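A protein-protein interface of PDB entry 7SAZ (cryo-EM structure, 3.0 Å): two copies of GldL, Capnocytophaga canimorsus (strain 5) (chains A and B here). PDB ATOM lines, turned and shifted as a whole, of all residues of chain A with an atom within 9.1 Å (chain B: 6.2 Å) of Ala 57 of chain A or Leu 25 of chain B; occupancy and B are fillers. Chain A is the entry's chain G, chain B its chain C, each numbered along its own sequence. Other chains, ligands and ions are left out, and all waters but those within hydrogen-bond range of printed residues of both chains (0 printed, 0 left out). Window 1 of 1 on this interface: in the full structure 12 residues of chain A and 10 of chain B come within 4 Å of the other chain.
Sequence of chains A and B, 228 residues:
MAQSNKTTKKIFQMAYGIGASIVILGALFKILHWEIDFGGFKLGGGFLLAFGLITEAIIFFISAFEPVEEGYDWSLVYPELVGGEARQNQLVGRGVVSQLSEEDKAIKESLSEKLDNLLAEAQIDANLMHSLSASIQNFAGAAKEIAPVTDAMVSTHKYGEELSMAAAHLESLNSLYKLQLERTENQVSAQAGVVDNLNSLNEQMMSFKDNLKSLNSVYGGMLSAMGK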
ATOM      1  N   ALA A  15     -15.527  37.572   1.266  1.00  0.00           N
ATOM      2  CA  ALA A  15     -14.961  36.620   2.212  1.00  0.00           C
ATOM      3  C   ALA A  15     -13.457  36.798   2.335  1.00  0.00           C
ATOM      4  O   ALA A  15     -12.911  36.736   3.439  1.00  0.00           O
ATOM      5  CB  ALA A  15     -15.299  35.193   1.789  1.00  0.00           C
ATOM      6  N   TYR A  16     -12.770  37.034   1.216  1.00  0.00           N
ATOM      7  CA  TYR A  16     -11.336  37.286   1.268  1.00  0.00           C
ATOM      8  C   TYR A  16     -11.033  38.525   2.095  1.00  0.00           C
ATOM      9  O   TYR A  16     -10.165  38.500   2.971  1.00  0.00           O
ATOM     10  CB  TYR A  16     -10.774  37.439  -0.145  1.00  0.00           C
ATOM     11  CG  TYR A  16      -9.351  37.948  -0.174  1.00  0.00           C
ATOM     12  CD1 TYR A  16      -8.323  37.218   0.403  1.00  0.00           C
ATOM     13  CD2 TYR A  16      -9.038  39.158  -0.770  1.00  0.00           C
ATOM     14  CE1 TYR A  16      -7.025  37.674   0.383  1.00  0.00           C
ATOM     15  CE2 TYR A  16      -7.740  39.624  -0.794  1.00  0.00           C
ATOM     16  CZ  TYR A  16      -6.738  38.877  -0.216  1.00  0.00           C
ATOM     17  OH  TYR A  16      -5.443  39.333  -0.236  1.00  0.00           O
ATOM     18  N   GLY A  19     -11.996  37.845   5.914  1.00  0.00           N
ATOM     19  CA  GLY A  19     -11.081  36.890   6.510  1.00  0.00           C
ATOM     20  C   GLY A  19      -9.677  37.438   6.656  1.00  0.00           C
ATOM     21  O   GLY A  19      -8.994  37.155   7.640  1.00  0.00           O
ATOM     22  N   ALA A  20      -9.224  38.234   5.683  1.00  0.00           N
ATOM     23  CA  ALA A  20      -7.915  38.862   5.795  1.00  0.00           C
ATOM     24  C   ALA A  20      -7.883  39.865   6.938  1.00  0.00           C
ATOM     25  O   ALA A  20      -6.911  39.912   7.706  1.00  0.00           O
ATOM     26  CB  ALA A  20      -7.545  39.534   4.478  1.00  0.00           C
ATOM     27  N   VAL A  23      -7.737  37.800  10.136  1.00  0.00           N
ATOM     28  CA  VAL A  23      -6.487  37.090  10.383  1.00  0.00           C
ATOM     29  C   VAL A  23      -5.373  38.060  10.749  1.00  0.00           C
ATOM     30  O   VAL A  23      -4.552  37.768  11.624  1.00  0.00           O
ATOM     31  CB  VAL A  23      -6.099  36.201   9.188  1.00  0.00           C
ATOM     32  CG1 VAL A  23      -5.822  37.016   7.967  1.00  0.00           C
ATOM     33  CG2 VAL A  23      -4.874  35.399   9.537  1.00  0.00           C
ATOM     34  N   LEU A  49      -6.687  34.193  14.477  1.00  0.00           N
ATOM     35  CA  LEU A  49      -5.798  33.651  13.456  1.00  0.00           C
ATOM     36  C   LEU A  49      -6.379  32.386  12.844  1.00  0.00           C
ATOM     37  O   LEU A  49      -6.389  32.226  11.621  1.00  0.00           O
ATOM     38  CB  LEU A  49      -4.421  33.370  14.054  1.00  0.00           C
ATOM     39  CG  LEU A  49      -3.375  34.475  13.962  1.00  0.00           C
ATOM     40  CD1 LEU A  49      -2.209  34.158  14.868  1.00  0.00           C
ATOM     41  CD2 LEU A  49      -2.904  34.636  12.533  1.00  0.00           C
ATOM     42  N   ALA A  50      -6.869  31.472  13.684  1.00  0.00           N
ATOM     43  CA  ALA A  50      -7.439  30.229  13.177  1.00  0.00           C
ATOM     44  C   ALA A  50      -8.639  30.504  12.287  1.00  0.00           C
ATOM     45  O   ALA A  50      -8.738  29.971  11.177  1.00  0.00           O
ATOM     46  CB  ALA A  50      -7.833  29.318  14.338  1.00  0.00           C
ATOM     47  N   PHE A  51      -9.552  31.359  12.748  1.00  0.00           N
ATOM     48  CA  PHE A  51     -10.742  31.671  11.966  1.00  0.00           C
ATOM     49  C   PHE A  51     -10.372  32.267  10.615  1.00  0.00           C
ATOM     50  O   PHE A  51     -10.822  31.789   9.565  1.00  0.00           O
ATOM     51  CB  PHE A  51     -11.640  32.625  12.752  1.00  0.00           C
ATOM     52  CG  PHE A  51     -13.012  32.779  12.173  1.00  0.00           C
ATOM     53  CD1 PHE A  51     -13.770  31.669  11.850  1.00  0.00           C
ATOM     54  CD2 PHE A  51     -13.546  34.035  11.957  1.00  0.00           C
ATOM     55  CE1 PHE A  51     -15.032  31.808  11.319  1.00  0.00           C
ATOM     56  CE2 PHE A  51     -14.809  34.181  11.425  1.00  0.00           C
ATOM     57  CZ  PHE A  51     -15.553  33.065  11.106  1.00  0.00           C
ATOM     58  N   GLY A  52      -9.531  33.304  10.620  1.00  0.00           N
ATOM     59  CA  GLY A  52      -9.181  33.962   9.373  1.00  0.00           C
ATOM     60  C   GLY A  52      -8.405  33.068   8.427  1.00  0.00           C
ATOM     61  O   GLY A  52      -8.687  33.029   7.228  1.00  0.00           O
ATOM     62  N   LEU A  53      -7.423  32.330   8.946  1.00  0.00           N
ATOM     63  CA  LEU A  53      -6.610  31.490   8.079  1.00  0.00           C
ATOM     64  C   LEU A  53      -7.418  30.330   7.513  1.00  0.00           C
ATOM     65  O   LEU A  53      -7.223  29.944   6.356  1.00  0.00           O
ATOM     66  CB  LEU A  53      -5.385  30.988   8.840  1.00  0.00           C
ATOM     67  CG  LEU A  53      -4.232  31.981   8.989  1.00  0.00           C
ATOM     68  CD1 LEU A  53      -3.060  31.363   9.718  1.00  0.00           C
ATOM     69  CD2 LEU A  53      -3.794  32.514   7.644  1.00  0.00           C
ATOM     70  N   ILE A  54      -8.344  29.770   8.297  1.00  0.00           N
ATOM     71  CA  ILE A  54      -9.197  28.708   7.777  1.00  0.00           C
ATOM     72  C   ILE A  54     -10.122  29.248   6.696  1.00  0.00           C
ATOM     73  O   ILE A  54     -10.277  28.639   5.631  1.00  0.00           O
ATOM     74  CB  ILE A  54      -9.986  28.042   8.917  1.00  0.00           C
ATOM     75  CG1 ILE A  54      -9.089  27.097   9.707  1.00  0.00           C
ATOM     76  CG2 ILE A  54     -11.172  27.277   8.367  1.00  0.00           C
ATOM     77  CD1 ILE A  54      -9.670  26.683  11.030  1.00  0.00           C
ATOM     78  N   THR A  55     -10.755  30.399   6.945  1.00  0.00           N
ATOM     79  CA  THR A  55     -11.659  30.928   5.932  1.00  0.00           C
ATOM     80  C   THR A  55     -10.921  31.502   4.731  1.00  0.00           C
ATOM     81  O   THR A  55     -11.561  31.795   3.719  1.00  0.00           O
ATOM     82  CB  THR A  55     -12.584  31.993   6.522  1.00  0.00           C
ATOM     83  OG1 THR A  55     -13.556  32.368   5.542  1.00  0.00           O
ATOM     84  CG2 THR A  55     -11.802  33.224   6.913  1.00  0.00           C
ATOM     85  N   GLU A  56      -9.604  31.679   4.820  1.00  0.00           N
ATOM     86  CA  GLU A  56      -8.812  32.036   3.650  1.00  0.00           C
ATOM     87  C   GLU A  56      -8.371  30.810   2.863  1.00  0.00           C
ATOM     88  O   GLU A  56      -8.425  30.814   1.628  1.00  0.00           O
ATOM     89  CB  GLU A  56      -7.585  32.848   4.069  1.00  0.00           C
ATOM     90  CG  GLU A  56      -7.898  34.267   4.482  1.00  0.00           C
ATOM     91  CD  GLU A  56      -8.586  35.044   3.389  1.00  0.00           C
ATOM     92  OE1 GLU A  56      -8.272  34.802   2.208  1.00  0.00           O
ATOM     93  OE2 GLU A  56      -9.441  35.892   3.710  1.00  0.00           O
ATOM     94  N   ALA A  57      -7.930  29.760   3.560  1.00  0.00           N
ATOM     95  CA  ALA A  57      -7.561  28.523   2.886  1.00  0.00           C
ATOM     96  C   ALA A  57      -8.757  27.912   2.170  1.00  0.00           C
ATOM     97  O   ALA A  57      -8.627  27.410   1.047  1.00  0.00           O
ATOM     98  CB  ALA A  57      -6.970  27.536   3.889  1.00  0.00           C
ATOM     99  N   ILE A  58      -9.933  27.947   2.801  1.00  0.00           N
ATOM    100  CA  ILE A  58     -11.135  27.424   2.159  1.00  0.00           C
ATOM    101  C   ILE A  58     -11.443  28.209   0.891  1.00  0.00           C
ATOM    102  O   ILE A  58     -11.727  27.632  -0.163  1.00  0.00           O
ATOM    103  CB  ILE A  58     -12.321  27.451   3.138  1.00  0.00           C
ATOM    104  CG1 ILE A  58     -12.209  26.308   4.145  1.00  0.00           C
ATOM    105  CG2 ILE A  58     -13.636  27.366   2.386  1.00  0.00           C
ATOM    106  CD1 ILE A  58     -13.186  26.416   5.287  1.00  0.00           C
ATOM    107  N   ILE A  59     -11.380  29.540   0.972  1.00  0.00           N
ATOM    108  CA  ILE A  59     -11.706  30.373  -0.185  1.00  0.00           C
ATOM    109  C   ILE A  59     -10.722  30.126  -1.320  1.00  0.00           C
ATOM    110  O   ILE A  59     -11.115  30.023  -2.488  1.00  0.00           O
ATOM    111  CB  ILE A  59     -11.748  31.858   0.217  1.00  0.00           C
ATOM    112  CG1 ILE A  59     -13.018  32.152   1.014  1.00  0.00           C
ATOM    113  CG2 ILE A  59     -11.664  32.749  -1.009  1.00  0.00           C
ATOM    114  CD1 ILE A  59     -14.281  31.670   0.348  1.00  0.00           C
ATOM    115  N   PHE A  60      -9.431  30.025  -1.000  1.00  0.00           N
ATOM    116  CA  PHE A  60      -8.442  29.787  -2.046  1.00  0.00           C
ATOM    117  C   PHE A  60      -8.584  28.397  -2.650  1.00  0.00           C
ATOM    118  O   PHE A  60      -8.342  28.220  -3.849  1.00  0.00           O
ATOM    119  CB  PHE A  60      -7.034  30.000  -1.497  1.00  0.00           C
ATOM    120  CG  PHE A  60      -6.675  31.444  -1.325  1.00  0.00           C
ATOM    121  CD1 PHE A  60      -6.955  32.362  -2.319  1.00  0.00           C
ATOM    122  CD2 PHE A  60      -6.077  31.889  -0.165  1.00  0.00           C
ATOM    123  CE1 PHE A  60      -6.635  33.691  -2.162  1.00  0.00           C
ATOM    124  CE2 PHE A  60      -5.756  33.219  -0.003  1.00  0.00           C
ATOM    125  CZ  PHE A  60      -6.035  34.119  -1.002  1.00  0.00           C
ATOM    126  N   PHE A  61      -8.967  27.403  -1.847  1.00  0.00           N
ATOM    127  CA  PHE A  61      -9.200  26.069  -2.389  1.00  0.00           C
ATOM    128  C   PHE A  61     -10.365  26.069  -3.370  1.00  0.00           C
ATOM    129  O   PHE A  61     -10.258  25.523  -4.474  1.00  0.00           O
ATOM    130  CB  PHE A  61      -9.454  25.078  -1.254  1.00  0.00           C
ATOM    131  CG  PHE A  61      -9.275  23.642  -1.651  1.00  0.00           C
ATOM    132  CD1 PHE A  61     -10.247  22.982  -2.383  1.00  0.00           C
ATOM    133  CD2 PHE A  61      -8.133  22.950  -1.290  1.00  0.00           C
ATOM    134  CE1 PHE A  61     -10.084  21.664  -2.748  1.00  0.00           C
ATOM    135  CE2 PHE A  61      -7.965  21.629  -1.653  1.00  0.00           C
ATOM    136  CZ  PHE A  61      -8.942  20.986  -2.384  1.00  0.00           C
ATOM    137  N   ILE A  62     -11.489  26.675  -2.986  1.00  0.00           N
ATOM    138  CA  ILE A  62     -12.672  26.657  -3.842  1.00  0.00           C
ATOM    139  C   ILE A  62     -12.437  27.486  -5.098  1.00  0.00           C
ATOM    140  O   ILE A  62     -12.895  27.126  -6.188  1.00  0.00           O
ATOM    141  CB  ILE A  62     -13.909  27.141  -3.066  1.00  0.00           C
ATOM    142  CG1 ILE A  62     -14.079  26.337  -1.779  1.00  0.00           C
ATOM    143  CG2 ILE A  62     -15.152  26.995  -3.916  1.00  0.00           C
ATOM    144  CD1 ILE A  62     -14.302  24.865  -2.009  1.00  0.00           C
ATOM    145  N   SER A  63     -11.721  28.604  -4.973  1.00  0.00           N
ATOM    146  CA  SER A  63     -11.455  29.454  -6.127  1.00  0.00           C
ATOM    147  C   SER A  63     -10.503  28.814  -7.128  1.00  0.00           C
ATOM    148  O   SER A  63     -10.352  29.340  -8.234  1.00  0.00           O
ATOM    149  CB  SER A  63     -10.889  30.799  -5.673  1.00  0.00           C
ATOM    150  OG  SER A  63     -10.596  31.624  -6.788  1.00  0.00           O
ATOM    151  N   ALA A  64      -9.855  27.707  -6.769  1.00  0.00           N
ATOM    152  CA  ALA A  64      -9.002  26.984  -7.702  1.00  0.00           C
ATOM    153  C   ALA A  64      -9.792  26.209  -8.746  1.00  0.00           C
ATOM    154  O   ALA A  64      -9.197  25.727  -9.714  1.00  0.00           O
ATOM    155  CB  ALA A  64      -8.085  26.024  -6.943  1.00  0.00           C
ATOM    156  N   PHE A  65     -11.102  26.076  -8.577  1.00  0.00           N
ATOM    157  CA  PHE A  65     -11.926  25.329  -9.515  1.00  0.00           C
ATOM    158  C   PHE A  65     -13.002  26.215 -10.130  1.00  0.00           C
ATOM    159  O   PHE A  65     -12.750  27.370 -10.470  1.00  0.00           O
ATOM    160  CB  PHE A  65     -12.567  24.128  -8.820  1.00  0.00           C
ATOM    161  CG  PHE A  65     -11.578  23.209  -8.165  1.00  0.00           C
ATOM    162  CD1 PHE A  65     -10.884  22.274  -8.910  1.00  0.00           C
ATOM    163  CD2 PHE A  65     -11.341  23.282  -6.805  1.00  0.00           C
ATOM    164  CE1 PHE A  65      -9.974  21.429  -8.310  1.00  0.00           C
ATOM    165  CE2 PHE A  65     -10.431  22.440  -6.200  1.00  0.00           C
ATOM    166  CZ  PHE A  65      -9.748  21.512  -6.954  1.00  0.00           C
ATOM    167  N   GLY B  17      -4.109  27.926  -6.631  1.00  0.00           N
ATOM    168  CA  GLY B  17      -5.048  27.880  -5.522  1.00  0.00           C
ATOM    169  C   GLY B  17      -4.725  26.795  -4.512  1.00  0.00           C
ATOM    170  O   GLY B  17      -4.772  27.028  -3.300  1.00  0.00           O
ATOM    171  N   ALA B  20      -1.689  27.744  -2.567  1.00  0.00           N
ATOM    172  CA  ALA B  20      -2.027  28.782  -1.603  1.00  0.00           C
ATOM    173  C   ALA B  20      -2.700  28.189  -0.378  1.00  0.00           C
ATOM    174  O   ALA B  20      -2.358  28.539   0.758  1.00  0.00           O
ATOM    175  CB  ALA B  20      -2.921  29.833  -2.254  1.00  0.00           C
ATOM    176  N   SER B  21      -3.648  27.277  -0.590  1.00  0.00           N
ATOM    177  CA  SER B  21      -4.300  26.631   0.541  1.00  0.00           C
ATOM    178  C   SER B  21      -3.295  25.865   1.388  1.00  0.00           C
ATOM    179  O   SER B  21      -3.324  25.947   2.621  1.00  0.00           O
ATOM    180  CB  SER B  21      -5.404  25.697   0.051  1.00  0.00           C
ATOM    181  OG  SER B  21      -6.559  26.430  -0.313  1.00  0.00           O
ATOM    182  N   ILE B  22      -2.382  25.132   0.745  1.00  0.00           N
ATOM    183  CA  ILE B  22      -1.412  24.338   1.494  1.00  0.00           C
ATOM    184  C   ILE B  22      -0.492  25.233   2.311  1.00  0.00           C
ATOM    185  O   ILE B  22      -0.203  24.943   3.477  1.00  0.00           O
ATOM    186  CB  ILE B  22      -0.613  23.426   0.545  1.00  0.00           C
ATOM    187  CG1 ILE B  22      -1.517  22.362  -0.065  1.00  0.00           C
ATOM    188  CG2 ILE B  22       0.539  22.771   1.280  1.00  0.00           C
ATOM    189  CD1 ILE B  22      -1.001  21.814  -1.367  1.00  0.00           C
ATOM    190  N   VAL B  23      -0.008  26.329   1.722  1.00  0.00           N
ATOM    191  CA  VAL B  23       0.941  27.167   2.447  1.00  0.00           C
ATOM    192  C   VAL B  23       0.240  27.907   3.581  1.00  0.00           C
ATOM    193  O   VAL B  23       0.802  28.071   4.670  1.00  0.00           O
ATOM    194  CB  VAL B  23       1.664  28.132   1.493  1.00  0.00           C
ATOM    195  CG1 VAL B  23       2.587  29.050   2.286  1.00  0.00           C
ATOM    196  CG2 VAL B  23       2.435  27.374   0.441  1.00  0.00           C
ATOM    197  N   ILE B  24      -0.995  28.363   3.351  1.00  0.00           N
ATOM    198  CA  ILE B  24      -1.747  29.011   4.421  1.00  0.00           C
ATOM    199  C   ILE B  24      -2.015  28.035   5.559  1.00  0.00           C
ATOM    200  O   ILE B  24      -1.911  28.394   6.736  1.00  0.00           O
ATOM    201  CB  ILE B  24      -3.049  29.622   3.873  1.00  0.00           C
ATOM    202  CG1 ILE B  24      -2.732  30.793   2.952  1.00  0.00           C
ATOM    203  CG2 ILE B  24      -3.942  30.075   4.999  1.00  0.00           C
ATOM    204  CD1 ILE B  24      -3.943  31.516   2.468  1.00  0.00           C
ATOM    205  N   LEU B  25      -2.355  26.785   5.235  1.00  0.00           N
ATOM    206  CA  LEU B  25      -2.605  25.804   6.286  1.00  0.00           C
ATOM    207  C   LEU B  25      -1.323  25.449   7.030  1.00  0.00           C
ATOM    208  O   LEU B  25      -1.347  25.221   8.243  1.00  0.00           O
ATOM    209  CB  LEU B  25      -3.252  24.555   5.695  1.00  0.00           C
ATOM    210  CG  LEU B  25      -4.736  24.699   5.359  1.00  0.00           C
ATOM    211  CD1 LEU B  25      -5.332  23.359   4.980  1.00  0.00           C
ATOM    212  CD2 LEU B  25      -5.486  25.315   6.524  1.00  0.00           C
ATOM    213  N   GLY B  26      -0.195  25.396   6.322  1.00  0.00           N
ATOM    214  CA  GLY B  26       1.074  25.187   6.997  1.00  0.00           C
ATOM    215  C   GLY B  26       1.409  26.315   7.952  1.00  0.00           C
ATOM    216  O   GLY B  26       1.862  26.078   9.074  1.00  0.00           O
ATOM    217  N   ALA B  27       1.178  27.558   7.526  1.00  0.00           N
ATOM    218  CA  ALA B  27       1.374  28.691   8.424  1.00  0.00           C
ATOM    219  C   ALA B  27       0.441  28.606   9.625  1.00  0.00           C
ATOM    220  O   ALA B  27       0.851  28.871  10.760  1.00  0.00           O
ATOM    221  CB  ALA B  27       1.162  30.003   7.672  1.00  0.00           C
ATOM    222  N   LEU B  28      -0.819  28.229   9.391  1.00  0.00           N
ATOM    223  CA  LEU B  28      -1.780  28.080  10.478  1.00  0.00           C
ATOM    224  C   LEU B  28      -1.297  27.065  11.503  1.00  0.00           C
ATOM    225  O   LEU B  28      -1.335  27.317  12.710  1.00  0.00           O
ATOM    226  CB  LEU B  28      -3.135  27.658   9.909  1.00  0.00           C
ATOM    227  CG  LEU B  28      -4.405  27.710  10.759  1.00  0.00           C
ATOM    228  CD1 LEU B  28      -5.601  27.682   9.850  1.00  0.00           C
ATOM    229  CD2 LEU B  28      -4.489  26.552  11.723  1.00  0.00           C
ATOM    230  N   PHE B  29      -0.847  25.901  11.036  1.00  0.00           N
ATOM    231  CA  PHE B  29      -0.438  24.857  11.965  1.00  0.00           C
ATOM    232  C   PHE B  29       0.884  25.188  12.641  1.00  0.00           C
ATOM    233  O   PHE B  29       1.138  24.721  13.755  1.00  0.00           O
ATOM    234  CB  PHE B  29      -0.350  23.516  11.242  1.00  0.00           C
ATOM    235  CG  PHE B  29      -1.675  22.833  11.072  1.00  0.00           C
ATOM    236  CD1 PHE B  29      -2.659  23.387  10.278  1.00  0.00           C
ATOM    237  CD2 PHE B  29      -1.935  21.638  11.709  1.00  0.00           C
ATOM    238  CE1 PHE B  29      -3.874  22.765  10.120  1.00  0.00           C
ATOM    239  CE2 PHE B  29      -3.150  21.009  11.554  1.00  0.00           C
ATOM    240  CZ  PHE B  29      -4.121  21.575  10.758  1.00  0.00           C
ATOM    241  N   LYS B  30       1.739  25.981  11.996  1.00  0.00           N
ATOM    242  CA  LYS B  30       2.982  26.378  12.645  1.00  0.00           C
ATOM    243  C   LYS B  30       2.734  27.431  13.717  1.00  0.00           C
ATOM    244  O   LYS B  30       3.366  27.404  14.779  1.00  0.00           O
ATOM    245  CB  LYS B  30       3.977  26.889  11.606  1.00  0.00           C
ATOM    246  CG  LYS B  30       5.252  27.456  12.198  1.00  0.00           C
ATOM    247  CD  LYS B  30       6.278  26.369  12.441  1.00  0.00           C
ATOM    248  CE  LYS B  30       7.528  26.933  13.089  1.00  0.00           C
ATOM    249  NZ  LYS B  30       8.252  25.906  13.883  1.00  0.00           N
ATOM    250  N   LEU B  48       4.283  20.418   8.715  1.00  0.00           N
ATOM    251  CA  LEU B  48       3.343  21.001   7.767  1.00  0.00           C
ATOM    252  C   LEU B  48       3.846  22.328   7.221  1.00  0.00           C
ATOM    253  O   LEU B  48       3.579  22.658   6.063  1.00  0.00           O
ATOM    254  CB  LEU B  48       1.973  21.169   8.415  1.00  0.00           C
ATOM    255  CG  LEU B  48       1.109  19.914   8.341  1.00  0.00           C
ATOM    256  CD1 LEU B  48       0.173  19.838   9.524  1.00  0.00           C
ATOM    257  CD2 LEU B  48       0.335  19.884   7.036  1.00  0.00           C
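O of Ala 57 of chain A sits at hydrogen-bond distance from OG of Ser 21 of chain B, 2.7 Å away. N of Phe 61 of chain A sits at hydrogen-bond distance from OG of Ser 21 of chain B, 3.0 Å away.
Among the printed residues, merely in contact across the chains: Leu 53 of chain A with Ile 24 of chain B, Leu 53 of chain A with Leu 28 of chain B, Ile 54 of chain A with Leu 28 of chain B, Ala 57 of chain A with Leu 25 of chain B, Phe 60 of chain A with Gly 17 of chain B, Phe 60 of chain A with Ser 21 of chain B, Phe 60 of chain A with Ile 24 of chain B and Ala 64 of chain A with Gly 17 of chain B.
Printed residues of chain B within 4 Å of Leu 53 of chain A: Ile 24 and Leu 28. Ala 57 of chain A touches two residues of chain B. Of the printed residues of chain B, Phe 60 of chain A touches Gly 17, Ser 21 and Ile 24. Of the printed residues of chain B, Phe 61 of chain A touches Ser 21. Ile 62 of chain A touches none of the printed residues of chain B. Of the printed residues of chain A, Gly 17 of chain B touches Phe 60 and Ala 64. Ile 22 of chain B touches none of the printed residues of chain A. Of chain A, only Ala 57 (3.8 Å) comes within 4 Å of Leu 25 of chain B. No residue of chain A comes within 4 Å of Gly 26 of chain B. The nearest residue of chain B that does not touch Ala 57 of chain A is Ile 24 of chain B (4.1 Å). The nearest residue of chain A that does not touch Leu 25 of chain B is Leu 53 of chain A (4.9 Å).
Printed residues of chain B that touch a printed residue of chain A: Gly 17, Ser 21, Ile 24, Leu 25 and Leu 28. Hydrophobic or aromatic side chains of chain B within 4 Å of the printed part of chain A: Ile 24, Leu 25 and Leu 28. Of the 22 printed residues of chain A, 6 touch a printed residue of chain B. Hydrophobic or aromatic side chains of chain A that line the printed part of chain B: Leu 53, Ile 54, Ala 57, Phe 60, Phe 61 and Ala 64. Among the printed residues, 10 pairs touch across the chains. Among the printed residues, no Asp or Glu carboxylate lies within 4 Å of a Lys or Arg side-chain nitrogen of the other chain.
Positions printed for both chains: 20 and 23. Of the 10 pairs that touch across the chains among the printed residues, none has its exchanged pair printed and touching as well.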
